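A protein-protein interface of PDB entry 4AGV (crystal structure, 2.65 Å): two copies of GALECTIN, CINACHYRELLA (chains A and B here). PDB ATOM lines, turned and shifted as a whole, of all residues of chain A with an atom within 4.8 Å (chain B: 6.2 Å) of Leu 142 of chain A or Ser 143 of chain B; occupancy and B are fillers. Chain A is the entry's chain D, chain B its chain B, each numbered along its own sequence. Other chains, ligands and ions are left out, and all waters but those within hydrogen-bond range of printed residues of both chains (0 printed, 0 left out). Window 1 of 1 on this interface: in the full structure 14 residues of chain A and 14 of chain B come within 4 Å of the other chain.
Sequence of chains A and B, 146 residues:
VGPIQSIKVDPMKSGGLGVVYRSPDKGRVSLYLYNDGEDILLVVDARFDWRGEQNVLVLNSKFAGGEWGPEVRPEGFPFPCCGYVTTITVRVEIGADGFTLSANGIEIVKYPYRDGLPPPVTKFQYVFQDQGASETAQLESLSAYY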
ATOM      1  N   GLN A   5      28.909   4.069 -21.193  1.00  0.00           N
ATOM      2  CA  GLN A   5      28.264   5.399 -21.201  1.00  0.00           C
ATOM      3  C   GLN A   5      28.660   6.238 -22.408  1.00  0.00           C
ATOM      4  O   GLN A   5      29.740   6.057 -22.949  1.00  0.00           O
ATOM      5  CB  GLN A   5      28.614   6.175 -19.922  1.00  0.00           C
ATOM      6  CG  GLN A   5      27.939   5.653 -18.672  1.00  0.00           C
ATOM      7  CD  GLN A   5      26.440   5.816 -18.742  1.00  0.00           C
ATOM      8  OE1 GLN A   5      25.712   5.233 -17.949  1.00  0.00           O
ATOM      9  NE2 GLN A   5      25.966   6.621 -19.699  1.00  0.00           N
ATOM     10  N   SER A   6      27.809   7.179 -22.808  1.00  0.00           N
ATOM     11  CA  SER A   6      28.108   7.978 -23.997  1.00  0.00           C
ATOM     12  C   SER A   6      27.537   9.392 -23.993  1.00  0.00           C
ATOM     13  O   SER A   6      26.630   9.707 -23.234  1.00  0.00           O
ATOM     14  CB  SER A   6      27.588   7.272 -25.243  1.00  0.00           C
ATOM     15  OG  SER A   6      26.201   7.518 -25.352  1.00  0.00           O
ATOM     16  N   ILE A   7      28.082  10.231 -24.871  1.00  0.00           N
ATOM     17  CA  ILE A   7      27.511  11.538 -25.186  1.00  0.00           C
ATOM     18  C   ILE A   7      27.404  11.724 -26.720  1.00  0.00           C
ATOM     19  O   ILE A   7      28.419  11.725 -27.444  1.00  0.00           O
ATOM     20  CB  ILE A   7      28.276  12.698 -24.494  1.00  0.00           C
ATOM     21  CG1 ILE A   7      29.768  12.647 -24.800  1.00  0.00           C
ATOM     22  CG2 ILE A   7      28.086  12.639 -22.981  1.00  0.00           C
ATOM     23  CD1 ILE A   7      30.452  13.991 -24.716  1.00  0.00           C
ATOM     24  N   GLY A  18      36.435  14.925 -23.839  1.00  0.00           N
ATOM     25  CA  GLY A  18      37.217  14.698 -22.630  1.00  0.00           C
ATOM     26  C   GLY A  18      36.526  13.718 -21.734  1.00  0.00           C
ATOM     27  O   GLY A  18      35.302  13.662 -21.719  1.00  0.00           O
ATOM     28  N   VAL A  19      37.318  12.923 -21.014  1.00  0.00           N
ATOM     29  CA  VAL A  19      36.787  11.932 -20.086  1.00  0.00           C
ATOM     30  C   VAL A  19      37.640  11.815 -18.818  1.00  0.00           C
ATOM     31  O   VAL A  19      38.844  11.982 -18.863  1.00  0.00           O
ATOM     32  CB  VAL A  19      36.627  10.564 -20.788  1.00  0.00           C
ATOM     33  CG1 VAL A  19      37.930  10.171 -21.484  1.00  0.00           C
ATOM     34  CG2 VAL A  19      36.131   9.499 -19.817  1.00  0.00           C
ATOM     35  N   PHE A 124      30.761   9.728 -28.563  1.00  0.00           N
ATOM     36  CA  PHE A 124      32.007   9.472 -27.839  1.00  0.00           C
ATOM     37  C   PHE A 124      31.571   8.589 -26.696  1.00  0.00           C
ATOM     38  O   PHE A 124      30.573   8.883 -26.052  1.00  0.00           O
ATOM     39  CB  PHE A 124      32.571  10.817 -27.355  1.00  0.00           C
ATOM     40  CG  PHE A 124      33.735  10.728 -26.400  1.00  0.00           C
ATOM     41  CD1 PHE A 124      34.984  10.253 -26.817  1.00  0.00           C
ATOM     42  CD2 PHE A 124      33.612  11.223 -25.100  1.00  0.00           C
ATOM     43  CE1 PHE A 124      36.071  10.234 -25.947  1.00  0.00           C
ATOM     44  CE2 PHE A 124      34.705  11.206 -24.226  1.00  0.00           C
ATOM     45  CZ  PHE A 124      35.934  10.710 -24.647  1.00  0.00           C
ATOM     46  N   TYR A 126      32.602   5.537 -23.509  1.00  0.00           N
ATOM     47  CA  TYR A 126      33.455   4.818 -22.566  1.00  0.00           C
ATOM     48  C   TYR A 126      32.943   3.396 -22.435  1.00  0.00           C
ATOM     49  O   TYR A 126      31.727   3.182 -22.318  1.00  0.00           O
ATOM     50  CB  TYR A 126      33.407   5.528 -21.210  1.00  0.00           C
ATOM     51  CG  TYR A 126      33.909   4.756 -19.996  1.00  0.00           C
ATOM     52  CD1 TYR A 126      33.125   3.767 -19.401  1.00  0.00           C
ATOM     53  CD2 TYR A 126      35.128   5.066 -19.391  1.00  0.00           C
ATOM     54  CE1 TYR A 126      33.551   3.078 -18.267  1.00  0.00           C
ATOM     55  CE2 TYR A 126      35.566   4.377 -18.256  1.00  0.00           C
ATOM     56  CZ  TYR A 126      34.771   3.383 -17.695  1.00  0.00           C
ATOM     57  OH  TYR A 126      35.168   2.679 -16.562  1.00  0.00           O
ATOM     58  N   LEU A 139      33.540   5.499 -13.931  1.00  0.00           N
ATOM     59  CA  LEU A 139      33.494   6.642 -14.792  1.00  0.00           C
ATOM     60  C   LEU A 139      33.167   7.865 -13.957  1.00  0.00           C
ATOM     61  O   LEU A 139      32.309   7.810 -13.075  1.00  0.00           O
ATOM     62  CB  LEU A 139      32.462   6.429 -15.892  1.00  0.00           C
ATOM     63  CG  LEU A 139      32.229   7.629 -16.816  1.00  0.00           C
ATOM     64  CD1 LEU A 139      33.503   8.035 -17.552  1.00  0.00           C
ATOM     65  CD2 LEU A 139      31.098   7.346 -17.794  1.00  0.00           C
ATOM     66  N   SER A 141      33.333  11.540 -15.482  1.00  0.00           N
ATOM     67  CA  SER A 141      32.742  12.540 -16.378  1.00  0.00           C
ATOM     68  C   SER A 141      32.981  12.246 -17.885  1.00  0.00           C
ATOM     69  O   SER A 141      33.919  11.516 -18.244  1.00  0.00           O
ATOM     70  CB  SER A 141      33.276  13.939 -16.030  1.00  0.00           C
ATOM     71  OG  SER A 141      34.608  14.146 -16.485  1.00  0.00           O
ATOM     72  N   LEU A 142      32.132  12.822 -18.746  1.00  0.00           N
ATOM     73  CA  LEU A 142      32.311  12.872 -20.217  1.00  0.00           C
ATOM     74  C   LEU A 142      32.020  14.290 -20.707  1.00  0.00           C
ATOM     75  O   LEU A 142      30.964  14.813 -20.383  1.00  0.00           O
ATOM     76  CB  LEU A 142      31.341  11.931 -20.932  1.00  0.00           C
ATOM     77  CG  LEU A 142      31.467  10.415 -20.876  1.00  0.00           C
ATOM     78  CD1 LEU A 142      30.701   9.827 -22.044  1.00  0.00           C
ATOM     79  CD2 LEU A 142      32.914   9.980 -20.966  1.00  0.00           C
ATOM     80  N   SER A 143      32.918  14.905 -21.484  1.00  0.00           N
ATOM     81  CA  SER A 143      32.750  16.302 -21.908  1.00  0.00           C
ATOM     82  C   SER A 143      32.920  16.590 -23.392  1.00  0.00           C
ATOM     83  O   SER A 143      33.747  15.992 -24.054  1.00  0.00           O
ATOM     84  CB  SER A 143      33.685  17.194 -21.134  1.00  0.00           C
ATOM     85  OG  SER A 143      33.275  17.191 -19.792  1.00  0.00           O
ATOM     86  N   ALA A 144      32.120  17.524 -23.888  1.00  0.00           N
ATOM     87  CA  ALA A 144      32.255  18.025 -25.227  1.00  0.00           C
ATOM     88  C   ALA A 144      32.843  19.433 -25.130  1.00  0.00           C
ATOM     89  O   ALA A 144      32.365  20.235 -24.334  1.00  0.00           O
ATOM     90  CB  ALA A 144      30.899  18.052 -25.894  1.00  0.00           C
ATOM     91  N   ILE B   7      24.055  17.817 -25.841  1.00  0.00           N
ATOM     92  CA  ILE B   7      24.564  16.456 -25.644  1.00  0.00           C
ATOM     93  C   ILE B   7      23.437  15.483 -25.198  1.00  0.00           C
ATOM     94  O   ILE B   7      22.535  15.863 -24.427  1.00  0.00           O
ATOM     95  CB  ILE B   7      25.768  16.448 -24.667  1.00  0.00           C
ATOM     96  CG1 ILE B   7      25.361  16.948 -23.278  1.00  0.00           C
ATOM     97  CG2 ILE B   7      26.898  17.316 -25.206  1.00  0.00           C
ATOM     98  CD1 ILE B   7      26.262  16.478 -22.166  1.00  0.00           C
ATOM     99  N   GLY B  16      24.943  14.426 -12.327  1.00  0.00           N
ATOM    100  CA  GLY B  16      24.675  15.861 -12.487  1.00  0.00           C
ATOM    101  C   GLY B  16      25.063  16.231 -13.909  1.00  0.00           C
ATOM    102  O   GLY B  16      25.586  15.373 -14.636  1.00  0.00           O
ATOM    103  N   LEU B  17      24.821  17.490 -14.298  1.00  0.00           N
ATOM    104  CA  LEU B  17      25.133  18.011 -15.637  1.00  0.00           C
ATOM    105  C   LEU B  17      25.747  19.425 -15.577  1.00  0.00           C
ATOM    106  O   LEU B  17      25.278  20.283 -14.820  1.00  0.00           O
ATOM    107  CB  LEU B  17      23.855  18.034 -16.485  1.00  0.00           C
ATOM    108  CG  LEU B  17      23.255  16.724 -17.042  1.00  0.00           C
ATOM    109  CD1 LEU B  17      21.748  16.698 -16.887  1.00  0.00           C
ATOM    110  CD2 LEU B  17      23.642  16.457 -18.491  1.00  0.00           C
ATOM    111  N   GLY B  18      26.772  19.692 -16.377  1.00  0.00           N
ATOM    112  CA  GLY B  18      27.390  21.029 -16.383  1.00  0.00           C
ATOM    113  C   GLY B  18      27.623  21.741 -17.716  1.00  0.00           C
ATOM    114  O   GLY B  18      27.702  21.111 -18.771  1.00  0.00           O
ATOM    115  N   VAL B  19      27.748  23.065 -17.650  1.00  0.00           N
ATOM    116  CA  VAL B  19      28.084  23.897 -18.807  1.00  0.00           C
ATOM    117  C   VAL B  19      29.019  25.036 -18.390  1.00  0.00           C
ATOM    118  O   VAL B  19      28.932  25.537 -17.269  1.00  0.00           O
ATOM    119  CB  VAL B  19      26.820  24.481 -19.487  1.00  0.00           C
ATOM    120  CG1 VAL B  19      25.969  25.281 -18.502  1.00  0.00           C
ATOM    121  CG2 VAL B  19      27.182  25.361 -20.672  1.00  0.00           C
ATOM    122  N   PHE B 124      20.376  17.442 -22.897  1.00  0.00           N
ATOM    123  CA  PHE B 124      20.740  18.667 -22.182  1.00  0.00           C
ATOM    124  C   PHE B 124      21.228  19.720 -23.147  1.00  0.00           C
ATOM    125  O   PHE B 124      22.253  19.539 -23.784  1.00  0.00           O
ATOM    126  CB  PHE B 124      21.823  18.364 -21.156  1.00  0.00           C
ATOM    127  CG  PHE B 124      22.338  19.573 -20.423  1.00  0.00           C
ATOM    128  CD1 PHE B 124      21.470  20.464 -19.820  1.00  0.00           C
ATOM    129  CD2 PHE B 124      23.709  19.787 -20.296  1.00  0.00           C
ATOM    130  CE1 PHE B 124      21.958  21.549 -19.128  1.00  0.00           C
ATOM    131  CE2 PHE B 124      24.199  20.881 -19.609  1.00  0.00           C
ATOM    132  CZ  PHE B 124      23.321  21.760 -19.018  1.00  0.00           C
ATOM    133  N   SER B 141      32.005  24.596 -22.962  1.00  0.00           N
ATOM    134  CA  SER B 141      31.884  23.164 -22.710  1.00  0.00           C
ATOM    135  C   SER B 141      30.480  22.680 -22.278  1.00  0.00           C
ATOM    136  O   SER B 141      29.619  23.484 -21.895  1.00  0.00           O
ATOM    137  CB  SER B 141      32.959  22.716 -21.707  1.00  0.00           C
ATOM    138  OG  SER B 141      32.628  23.105 -20.392  1.00  0.00           O
ATOM    139  N   LEU B 142      30.255  21.366 -22.386  1.00  0.00           N
ATOM    140  CA  LEU B 142      29.071  20.696 -21.847  1.00  0.00           C
ATOM    141  C   LEU B 142      29.581  19.386 -21.273  1.00  0.00           C
ATOM    142  O   LEU B 142      30.415  18.724 -21.906  1.00  0.00           O
ATOM    143  CB  LEU B 142      28.027  20.395 -22.928  1.00  0.00           C
ATOM    144  CG  LEU B 142      27.225  21.506 -23.615  1.00  0.00           C
ATOM    145  CD1 LEU B 142      26.281  20.953 -24.676  1.00  0.00           C
ATOM    146  CD2 LEU B 142      26.431  22.339 -22.625  1.00  0.00           C
ATOM    147  N   SER B 143      29.108  19.024 -20.079  1.00  0.00           N
ATOM    148  CA  SER B 143      29.623  17.847 -19.370  1.00  0.00           C
ATOM    149  C   SER B 143      28.529  17.065 -18.682  1.00  0.00           C
ATOM    150  O   SER B 143      27.601  17.658 -18.137  1.00  0.00           O
ATOM    151  CB  SER B 143      30.664  18.243 -18.313  1.00  0.00           C
ATOM    152  OG  SER B 143      31.686  19.081 -18.828  1.00  0.00           O
ATOM    153  N   ALA B 144      28.655  15.734 -18.709  1.00  0.00           N
ATOM    154  CA  ALA B 144      27.806  14.832 -17.933  1.00  0.00           C
ATOM    155  C   ALA B 144      28.647  14.132 -16.870  1.00  0.00           C
ATOM    156  O   ALA B 144      29.769  13.703 -17.148  1.00  0.00           O
ATOM    157  CB  ALA B 144      27.151  13.812 -18.838  1.00  0.00           C
ATOM    158  N   TYR B 145      28.081  14.021 -15.662  1.00  0.00           N
ATOM    159  CA  TYR B 145      28.785  13.524 -14.488  1.00  0.00           C
ATOM    160  C   TYR B 145      28.180  12.281 -13.917  1.00  0.00           C
ATOM    161  O   TYR B 145      26.965  12.192 -13.703  1.00  0.00           O
ATOM    162  CB  TYR B 145      28.807  14.572 -13.389  1.00  0.00           C
ATOM    163  CG  TYR B 145      29.564  15.787 -13.782  1.00  0.00           C
ATOM    164  CD1 TYR B 145      30.962  15.762 -13.864  1.00  0.00           C
ATOM    165  CD2 TYR B 145      28.891  16.966 -14.098  1.00  0.00           C
ATOM    166  CE1 TYR B 145      31.674  16.882 -14.248  1.00  0.00           C
ATOM    167  CE2 TYR B 145      29.592  18.095 -14.479  1.00  0.00           C
ATOM    168  CZ  TYR B 145      30.979  18.041 -14.554  1.00  0.00           C
ATOM    169  OH  TYR B 145      31.665  19.166 -14.941  1.00  0.00           O
ATOM    170  N   TYR B 146      29.068  11.343 -13.615  1.00  0.00           N
ATOM    171  CA  TYR B 146      28.690  10.056 -13.107  1.00  0.00           C
ATOM    172  C   TYR B 146      29.439   9.833 -11.793  1.00  0.00           C
ATOM    173  O   TYR B 146      28.979   9.097 -10.920  1.00  0.00           O
ATOM    174  CB  TYR B 146      29.033   8.990 -14.154  1.00  0.00           C
ATOM    175  CG  TYR B 146      28.542   9.334 -15.540  1.00  0.00           C
ATOM    176  CD1 TYR B 146      27.268   8.962 -15.964  1.00  0.00           C
ATOM    177  CD2 TYR B 146      29.354  10.040 -16.428  1.00  0.00           C
ATOM    178  CE1 TYR B 146      26.807   9.281 -17.234  1.00  0.00           C
ATOM    179  CE2 TYR B 146      28.908  10.375 -17.692  1.00  0.00           C
ATOM    180  CZ  TYR B 146      27.626   9.991 -18.096  1.00  0.00           C
ATOM    181  OH  TYR B 146      27.197  10.325 -19.373  1.00  0.00           O
ATOM    182  OXT TYR B 146      30.519  10.402 -11.582  1.00  0.00           O
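The backbone carbonyl oxygen (O) of Leu 142 of chain B sits at hydrogen-bond distance from the backbone NH (N) of Ala 144 of chain A (2.9 Å).
The side-chain hydroxyl of Ser 143 of chain B sits at hydrogen-bond distance from the side-chain hydroxyl of Ser 143 of chain A.
O of Ala 144 of chain B lies within hydrogen-bond range of N of Leu 142 of chain A, at 3.0 Å.
OXT of Tyr 146 of chain B lies close to O of Leu 139 of chain A.
Of the printed residues of chain B, Ser 141 of chain A touches Ala 144 (3.3 Å) and Tyr 145 (3.7 Å).
Of chain B, only Ser 143 (3.5 Å) and Ala 144 (3.0 Å) come within 4 Å of Leu 142 of chain A.
Leu 17 of chain B touches none of the printed residues of chain A.
Of the printed residues of chain A, Ser 141 of chain B touches Ala 144.
Of the printed residues of chain A, Leu 142 of chain B touches Ser 143 and Ala 144.
Of chain A, only Leu 142 and Ser 143 come within 4 Å of Ser 143 of chain B.
Among the printed residues, merely in contact across the chains: Ser 141 of chain A with Ala 144 of chain B (3.3 Å), Ser 143 of chain A with Leu 142 of chain B (3.4 Å), Ala 144 of chain A with Ser 141 of chain B (3.4 Å), Leu 142 of chain A with Ser 143 of chain B (3.5 Å), Ser 141 of chain A with Tyr 145 of chain B (3.7 Å), Gln 5 of chain A with Tyr 146 of chain B (3.7 Å) and Ser 6 of chain A with Tyr 146 of chain B (3.95 Å).
The backbone NH (N) of Tyr 145 of chain B is in hydrogen-bond range of the backbone carbonyl oxygen (O) of Gly 16 of chain B (3.0 Å).
N of Gly 18 of chain B sits at hydrogen-bond distance from O of Ser 143 of chain B, 2.8 Å away.
O of Gln 5 of chain A lies within hydrogen-bond range of N of Tyr 126 of chain A, 3.0 Å away.
O of Gly 18 of chain A is in hydrogen-bond range of N of Ser 143 of chain A.
Of the 12 printed residues of chain A, 7 touch a printed residue of chain B.
Hydrophobic or aromatic side chains of chain A within 4 Å of the printed part of chain B: Leu 139.
Among the printed residues, 11 pairs touch across the chains.
Among the printed residues, no Asp or Glu carboxylate lies within 4 Å of a Lys or Arg side-chain nitrogen of the other chain.
Ser 141 of chain A touches Ala 144 of chain B, and with the chains exchanged Ala 144 of chain A touches Ser 141 of chain B.
Leu 142 of chain A touches Ser 143 of chain B, and with the chains exchanged Ser 143 of chain A touches Leu 142 of chain B.
Leu 142 of chain A touches Ala 144 of chain B, and with the chains exchanged Ala 144 of chain A touches Leu 142 of chain B.
Ser 143 of chain A touches its own counterpart, Ser 143 of chain B.
Positions printed for both chains: 7, 18, 19, 124, 141, 142, 143 and 144.
Of the 11 pairs that touch across the chains among the printed residues, 7 have their exchanged pair printed and touching as well.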
